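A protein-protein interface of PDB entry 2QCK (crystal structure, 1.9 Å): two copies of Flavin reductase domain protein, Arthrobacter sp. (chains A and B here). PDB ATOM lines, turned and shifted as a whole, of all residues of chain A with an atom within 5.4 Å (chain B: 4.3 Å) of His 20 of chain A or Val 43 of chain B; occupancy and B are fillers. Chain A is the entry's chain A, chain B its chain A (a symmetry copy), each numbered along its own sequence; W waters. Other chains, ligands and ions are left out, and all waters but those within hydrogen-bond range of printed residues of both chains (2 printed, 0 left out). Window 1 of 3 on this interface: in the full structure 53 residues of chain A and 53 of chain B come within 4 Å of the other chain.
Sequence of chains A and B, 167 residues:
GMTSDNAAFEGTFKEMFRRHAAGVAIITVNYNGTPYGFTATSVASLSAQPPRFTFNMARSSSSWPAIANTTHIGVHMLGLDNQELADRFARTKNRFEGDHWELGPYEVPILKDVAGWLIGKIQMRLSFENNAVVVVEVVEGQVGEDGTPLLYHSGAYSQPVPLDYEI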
ATOM      1  N   GLU A  15      30.777  -6.275  25.979  1.00  0.00           N
ATOM      2  CA  GLU A  15      30.412  -5.672  24.704  1.00  0.00           C
ATOM      3  C   GLU A  15      28.903  -5.510  24.551  1.00  0.00           C
ATOM      4  O   GLU A  15      28.447  -4.428  24.285  1.00  0.00           O
ATOM      5  CB  GLU A  15      30.995  -6.521  23.547  1.00  0.00           C
ATOM      6  CG  GLU A  15      30.718  -6.067  22.099  1.00  0.00           C
ATOM      7  CD  GLU A  15      31.108  -4.608  21.814  1.00  0.00           C
ATOM      8  OE1 GLU A  15      31.738  -3.930  22.676  1.00  0.00           O
ATOM      9  OE2 GLU A  15      30.736  -4.137  20.717  1.00  0.00           O
ATOM     10  N   MET A  16      28.132  -6.580  24.728  1.00  0.00           N
ATOM     11  CA  MET A  16      26.682  -6.498  24.547  1.00  0.00           C
ATOM     12  C   MET A  16      26.059  -5.432  25.450  1.00  0.00           C
ATOM     13  O   MET A  16      25.124  -4.763  25.023  1.00  0.00           O
ATOM     14  CB  MET A  16      25.989  -7.857  24.731  1.00  0.00           C
ATOM     15  CG  MET A  16      26.185  -8.872  23.629  1.00  0.00           C
ATOM     16  SD  MET A  16      26.291  -8.051  21.808  1.00  0.00           S
ATOM     17  CE  MET A  16      24.502  -7.156  21.862  1.00  0.00           C
ATOM     18  N   PHE A  17      26.555  -5.235  26.670  1.00  0.00           N
ATOM     19  CA  PHE A  17      26.020  -4.153  27.528  1.00  0.00           C
ATOM     20  C   PHE A  17      26.559  -2.771  27.177  1.00  0.00           C
ATOM     21  O   PHE A  17      25.951  -1.758  27.564  1.00  0.00           O
ATOM     22  CB  PHE A  17      26.119  -4.442  29.066  1.00  0.00           C
ATOM     23  CG  PHE A  17      25.030  -5.319  29.533  1.00  0.00           C
ATOM     24  CD1 PHE A  17      23.770  -4.806  29.741  1.00  0.00           C
ATOM     25  CD2 PHE A  17      25.217  -6.689  29.596  1.00  0.00           C
ATOM     26  CE1 PHE A  17      22.731  -5.630  30.057  1.00  0.00           C
ATOM     27  CE2 PHE A  17      24.180  -7.531  29.921  1.00  0.00           C
ATOM     28  CZ  PHE A  17      22.937  -6.998  30.147  1.00  0.00           C
ATOM     29  N   ARG A  18      27.699  -2.729  26.478  1.00  0.00           N
ATOM     30  CA  ARG A  18      28.138  -1.497  25.806  1.00  0.00           C
ATOM     31  C   ARG A  18      27.127  -1.077  24.752  1.00  0.00           C
ATOM     32  O   ARG A  18      26.916   0.089  24.520  1.00  0.00           O
ATOM     33  CB  ARG A  18      29.501  -1.696  25.131  1.00  0.00           C
ATOM     34  CG  ARG A  18      30.162  -0.401  24.646  1.00  0.00           C
ATOM     35  CD  ARG A  18      31.393  -0.601  23.725  1.00  0.00           C
ATOM     36  NE  ARG A  18      31.073  -1.286  22.466  1.00  0.00           N
ATOM     37  CZ  ARG A  18      30.398  -0.737  21.456  1.00  0.00           C
ATOM     38  NH1 ARG A  18      29.983   0.527  21.500  1.00  0.00           N
ATOM     39  NH2 ARG A  18      30.143  -1.453  20.371  1.00  0.00           N
ATOM     40  N   ARG A  19      26.504  -2.051  24.109  1.00  0.00           N
ATOM     41  CA  ARG A  19      25.548  -1.794  23.047  1.00  0.00           C
ATOM     42  C   ARG A  19      24.121  -1.583  23.527  1.00  0.00           C
ATOM     43  O   ARG A  19      23.203  -1.384  22.708  1.00  0.00           O
ATOM     44  CB  ARG A  19      25.563  -2.964  22.074  1.00  0.00           C
ATOM     45  CG  ARG A  19      26.889  -3.154  21.335  1.00  0.00           C
ATOM     46  CD  ARG A  19      26.723  -4.168  20.226  1.00  0.00           C
ATOM     47  NE  ARG A  19      28.022  -4.396  19.613  1.00  0.00           N
ATOM     48  CZ  ARG A  19      28.218  -5.046  18.476  1.00  0.00           C
ATOM     49  NH1 ARG A  19      27.202  -5.551  17.779  1.00  0.00           N
ATOM     50  NH2 ARG A  19      29.458  -5.189  18.026  1.00  0.00           N
ATOM     51  N   HIS A  20      23.914  -1.647  24.833  1.00  0.00           N
ATOM     52  CA  HIS A  20      22.591  -1.533  25.398  1.00  0.00           C
ATOM     53  C   HIS A  20      22.519  -0.148  26.033  1.00  0.00           C
ATOM     54  O   HIS A  20      23.270   0.135  26.958  1.00  0.00           O
ATOM     55  CB  HIS A  20      22.428  -2.642  26.435  1.00  0.00           C
ATOM     56  CG  HIS A  20      21.056  -2.758  26.995  1.00  0.00           C
ATOM     57  ND1 HIS A  20      19.963  -3.090  26.216  1.00  0.00           N
ATOM     58  CD2 HIS A  20      20.589  -2.604  28.254  1.00  0.00           C
ATOM     59  CE1 HIS A  20      18.882  -3.127  26.976  1.00  0.00           C
ATOM     60  NE2 HIS A  20      19.231  -2.843  28.218  1.00  0.00           N
ATOM     61  N   ALA A  21      21.639   0.721  25.542  1.00  0.00           N
ATOM     62  CA  ALA A  21      21.519   2.082  26.084  1.00  0.00           C
ATOM     63  C   ALA A  21      20.696   2.079  27.379  1.00  0.00           C
ATOM     64  O   ALA A  21      20.003   1.104  27.720  1.00  0.00           O
ATOM     65  CB  ALA A  21      20.862   2.984  25.058  1.00  0.00           C
ATOM     66  N   ALA A  22      20.721   3.186  28.112  1.00  0.00           N
ATOM     67  CA  ALA A  22      20.037   3.220  29.392  1.00  0.00           C
ATOM     68  C   ALA A  22      19.689   4.653  29.785  1.00  0.00           C
ATOM     69  O   ALA A  22      20.379   5.569  29.383  1.00  0.00           O
ATOM     70  CB  ALA A  22      20.931   2.582  30.450  1.00  0.00           C
ATOM     71  N   TYR A 152      22.466   7.243  28.661  1.00  0.00           N
ATOM     72  CA  TYR A 152      23.895   6.947  28.642  1.00  0.00           C
ATOM     73  C   TYR A 152      24.105   5.703  27.816  1.00  0.00           C
ATOM     74  O   TYR A 152      23.392   4.719  27.964  1.00  0.00           O
ATOM     75  CB  TYR A 152      24.355   6.664  30.019  1.00  0.00           C
ATOM     76  CG  TYR A 152      25.833   6.597  30.179  1.00  0.00           C
ATOM     77  CD1 TYR A 152      26.586   7.740  30.179  1.00  0.00           C
ATOM     78  CD2 TYR A 152      26.500   5.372  30.337  1.00  0.00           C
ATOM     79  CE1 TYR A 152      27.924   7.698  30.351  1.00  0.00           C
ATOM     80  CE2 TYR A 152      27.886   5.332  30.503  1.00  0.00           C
ATOM     81  CZ  TYR A 152      28.570   6.501  30.503  1.00  0.00           C
ATOM     82  OH  TYR A 152      29.939   6.517  30.679  1.00  0.00           O
ATOM     83  N   HIS A 153      25.064   5.757  26.916  1.00  0.00           N
ATOM     84  CA  HIS A 153      25.252   4.694  25.970  1.00  0.00           C
ATOM     85  C   HIS A 153      26.716   4.716  25.563  1.00  0.00           C
ATOM     86  O   HIS A 153      27.278   5.795  25.290  1.00  0.00           O
ATOM     87  CB  HIS A 153      24.364   4.927  24.753  1.00  0.00           C
ATOM     88  CG  HIS A 153      24.843   4.239  23.527  1.00  0.00           C
ATOM     89  ND1 HIS A 153      25.231   2.912  23.524  1.00  0.00           N
ATOM     90  CD2 HIS A 153      25.039   4.694  22.270  1.00  0.00           C
ATOM     91  CE1 HIS A 153      25.634   2.573  22.310  1.00  0.00           C
ATOM     92  NE2 HIS A 153      25.524   3.635  21.530  1.00  0.00           N
ATOM     93  N   GLY B  23      16.760   1.314  27.238  1.00  0.00           N
ATOM     94  CA  GLY B  23      17.094   0.536  26.069  1.00  0.00           C
ATOM     95  C   GLY B  23      16.137  -0.603  25.895  1.00  0.00           C
ATOM     96  O   GLY B  23      15.506  -1.009  26.840  1.00  0.00           O
ATOM     97  N   VAL B  24      16.085  -1.177  24.692  1.00  0.00           N
ATOM     98  CA  VAL B  24      15.089  -2.197  24.365  1.00  0.00           C
ATOM     99  C   VAL B  24      15.833  -3.490  24.051  1.00  0.00           C
ATOM    100  O   VAL B  24      16.741  -3.477  23.223  1.00  0.00           O
ATOM    101  CB  VAL B  24      14.172  -1.734  23.186  1.00  0.00           C
ATOM    102  CG1 VAL B  24      13.050  -2.770  22.893  1.00  0.00           C
ATOM    103  CG2 VAL B  24      13.573  -0.346  23.498  1.00  0.00           C
ATOM    104  N   ALA B  25      15.472  -4.571  24.759  1.00  0.00           N
ATOM    105  CA  ALA B  25      15.961  -5.922  24.496  1.00  0.00           C
ATOM    106  C   ALA B  25      14.755  -6.852  24.287  1.00  0.00           C
ATOM    107  O   ALA B  25      13.646  -6.451  24.545  1.00  0.00           O
ATOM    108  CB  ALA B  25      16.842  -6.416  25.690  1.00  0.00           C
ATOM    109  N   ALA B  40      11.409  -6.096  26.361  1.00  0.00           N
ATOM    110  CA  ALA B  40      11.681  -5.734  27.725  1.00  0.00           C
ATOM    111  C   ALA B  40      12.517  -4.452  27.764  1.00  0.00           C
ATOM    112  O   ALA B  40      13.417  -4.249  26.969  1.00  0.00           O
ATOM    113  CB  ALA B  40      12.443  -6.842  28.425  1.00  0.00           C
ATOM    114  N   THR B  41      12.161  -3.562  28.662  1.00  0.00           N
ATOM    115  CA  THR B  41      12.963  -2.361  28.910  1.00  0.00           C
ATOM    116  C   THR B  41      13.720  -2.380  30.245  1.00  0.00           C
ATOM    117  O   THR B  41      14.351  -1.380  30.606  1.00  0.00           O
ATOM    118  CB  THR B  41      12.068  -1.113  28.863  1.00  0.00           C
ATOM    119  OG1 THR B  41      10.884  -1.354  29.629  1.00  0.00           O
ATOM    120  CG2 THR B  41      11.642  -0.796  27.414  1.00  0.00           C
ATOM    121  N   SER B  42      13.721  -3.489  30.969  1.00  0.00           N
ATOM    122  CA  SER B  42      14.358  -3.508  32.304  1.00  0.00           C
ATOM    123  C   SER B  42      15.652  -4.297  32.408  1.00  0.00           C
ATOM    124  O   SER B  42      16.204  -4.475  33.500  1.00  0.00           O
ATOM    125  CB  SER B  42      13.368  -4.028  33.339  1.00  0.00           C
ATOM    126  OG  SER B  42      12.870  -5.317  33.007  1.00  0.00           O
ATOM    127  N   VAL B  43      16.160  -4.756  31.288  1.00  0.00           N
ATOM    128  CA  VAL B  43      17.310  -5.621  31.300  1.00  0.00           C
ATOM    129  C   VAL B  43      18.454  -4.724  31.765  1.00  0.00           C
ATOM    130  O   VAL B  43      18.569  -3.618  31.252  1.00  0.00           O
ATOM    131  CB  VAL B  43      17.601  -6.210  29.899  1.00  0.00           C
ATOM    132  CG1 VAL B  43      18.956  -6.837  29.863  1.00  0.00           C
ATOM    133  CG2 VAL B  43      16.504  -7.260  29.489  1.00  0.00           C
ATOM    134  N   ALA B  44      19.251  -5.192  32.721  1.00  0.00           N
ATOM    135  CA  ALA B  44      20.390  -4.422  33.303  1.00  0.00           C
ATOM    136  C   ALA B  44      21.456  -5.406  33.643  1.00  0.00           C
ATOM    137  O   ALA B  44      21.184  -6.516  34.097  1.00  0.00           O
ATOM    138  CB  ALA B  44      19.984  -3.704  34.543  1.00  0.00           C
ATOM    139  N   PHE B  53      22.791 -10.720  34.500  1.00  0.00           N
ATOM    140  CA  PHE B  53      21.911  -9.605  34.251  1.00  0.00           C
ATOM    141  C   PHE B  53      20.596  -9.883  34.945  1.00  0.00           C
ATOM    142  O   PHE B  53      20.336 -11.001  35.342  1.00  0.00           O
ATOM    143  CB  PHE B  53      21.669  -9.309  32.741  1.00  0.00           C
ATOM    144  CG  PHE B  53      20.951 -10.397  31.969  1.00  0.00           C
ATOM    145  CD1 PHE B  53      21.655 -11.397  31.344  1.00  0.00           C
ATOM    146  CD2 PHE B  53      19.579 -10.340  31.762  1.00  0.00           C
ATOM    147  CE1 PHE B  53      21.018 -12.365  30.605  1.00  0.00           C
ATOM    148  CE2 PHE B  53      18.941 -11.331  31.039  1.00  0.00           C
ATOM    149  CZ  PHE B  53      19.665 -12.321  30.461  1.00  0.00           C
ATOM    150  N   THR B  54      19.807  -8.829  35.094  1.00  0.00           N
ATOM    151  CA  THR B  54      18.488  -8.898  35.711  1.00  0.00           C
ATOM    152  C   THR B  54      17.455  -8.268  34.795  1.00  0.00           C
ATOM    153  O   THR B  54      17.795  -7.412  33.995  1.00  0.00           O
ATOM    154  CB  THR B  54      18.502  -8.108  37.024  1.00  0.00           C
ATOM    155  OG1 THR B  54      19.009  -6.800  36.769  1.00  0.00           O
ATOM    156  CG2 THR B  54      19.386  -8.769  38.037  1.00  0.00           C
ATOM    157  N   PHE B  55      16.199  -8.706  34.908  1.00  0.00           N
ATOM    158  CA  PHE B  55      15.070  -7.960  34.383  1.00  0.00           C
ATOM    159  C   PHE B  55      13.845  -8.202  35.270  1.00  0.00           C
ATOM    160  O   PHE B  55      13.835  -9.113  36.123  1.00  0.00           O
ATOM    161  CB  PHE B  55      14.798  -8.355  32.913  1.00  0.00           C
ATOM    162  CG  PHE B  55      14.407  -9.787  32.728  1.00  0.00           C
ATOM    163  CD1 PHE B  55      15.369 -10.781  32.672  1.00  0.00           C
ATOM    164  CD2 PHE B  55      13.049 -10.171  32.634  1.00  0.00           C
ATOM    165  CE1 PHE B  55      14.997 -12.105  32.477  1.00  0.00           C
ATOM    166  CE2 PHE B  55      12.706 -11.492  32.486  1.00  0.00           C
ATOM    167  CZ  PHE B  55      13.673 -12.456  32.418  1.00  0.00           C
ATOM    168  N   VAL B  75      18.698 -13.315  25.789  1.00  0.00           N
ATOM    169  CA  VAL B  75      18.417 -11.897  25.686  1.00  0.00           C
ATOM    170  C   VAL B  75      19.041 -11.289  24.424  1.00  0.00           C
ATOM    171  O   VAL B  75      20.187 -11.609  24.071  1.00  0.00           O
ATOM    172  CB  VAL B  75      18.846 -11.094  27.001  1.00  0.00           C
ATOM    173  CG1 VAL B  75      20.314 -11.095  27.200  1.00  0.00           C
ATOM    174  CG2 VAL B  75      18.296  -9.669  26.959  1.00  0.00           C
ATOM    175  N   MET B  77      19.879  -7.733  22.329  1.00  0.00           N
ATOM    176  CA  MET B  77      20.016  -6.263  22.260  1.00  0.00           C
ATOM    177  C   MET B  77      19.638  -5.868  20.844  1.00  0.00           C
ATOM    178  O   MET B  77      19.962  -6.574  19.879  1.00  0.00           O
ATOM    179  CB  MET B  77      21.452  -5.843  22.539  1.00  0.00           C
ATOM    180  CG  MET B  77      21.779  -5.813  24.008  1.00  0.00           C
ATOM    181  SD  MET B  77      21.739  -7.568  24.917  1.00  0.00           S
ATOM    182  CE  MET B  77      22.379  -6.910  26.704  1.00  0.00           C
HETATM  183  O   HOH W   1      17.994   0.292  29.767  1.00  0.00           O
HETATM  184  O   HOH W   2      19.326  -3.182  23.534  1.00  0.00           O
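A ring nitrogen (NE2) of His 20 of chain A lies within hydrogen-bond range of the backbone carbonyl oxygen (O) of Val 43 of chain B (3.2 Å). The backbone NH (N) of Gly 23 of chain B sits at hydrogen-bond distance from the backbone carbonyl oxygen (O) of Ala 21 of chain A (3.3 Å).
The backbone carbonyl oxygen (O) of Ala 44 of chain B is in hydrogen-bond range of the backbone NH (N) of Thr 54 of chain B (2.9 Å).
Among the printed residues, merely in contact across the chains: Met 16 of chain A with Met 77 of chain B, Phe 17 of chain A with Met 77 of chain B, Phe 17 of chain A with Phe 53 of chain B, Phe 17 of chain A with Ala 44 of chain B, His 20 of chain A with Gly 23 of chain B, His 20 of chain A with Met 77 of chain B and Phe 17 of chain A with Val 43 of chain B.
Of chain B, only Gly 23 (3.9 Å), Val 43 (3.2 Å) and Met 77 (3.9 Å) come within 4 Å of His 20 of chain A. Printed residues of chain A within 4 Å of Gly 23 of chain B: His 20 (3.9 Å) and Ala 21 (3.3 Å). Ser 42 of chain B touches none of the printed residues of chain A. Val 43 of chain B touches two residues of chain A. Of the printed residues of chain A, Ala 44 of chain B touches Phe 17. Of the printed residues of chain A, Phe 53 of chain B touches Phe 17.
Of the 10 printed residues of chain A, 4 touch a printed residue of chain B. Printed residues of chain A that touch a printed residue of chain B: Met 16, Phe 17, His 20 and Ala 21. Hydrophobic or aromatic side chains of chain A that line the printed part of chain B: Met 16, Phe 17 and His 20. Of the 13 printed residues of chain B, 5 touch a printed residue of chain A. Hydrophobic or aromatic side chains of chain B that line the printed part of chain A: Val 43, Phe 53 and Met 77. Along chain B the printed residues that touch a printed residue of chain A span positions 23 to 77. Among the printed residues, 9 pairs touch across the chains.
No position is printed for both chains.
Water W2 bridges the backbone carbonyl oxygen (O) of Val 24 of chain B and a ring nitrogen (ND1) of His 20 of chain A. Water W1 bridges the backbone carbonyl oxygen of Ala 21 of chain A and the backbone NH of Gly 23 of chain B.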
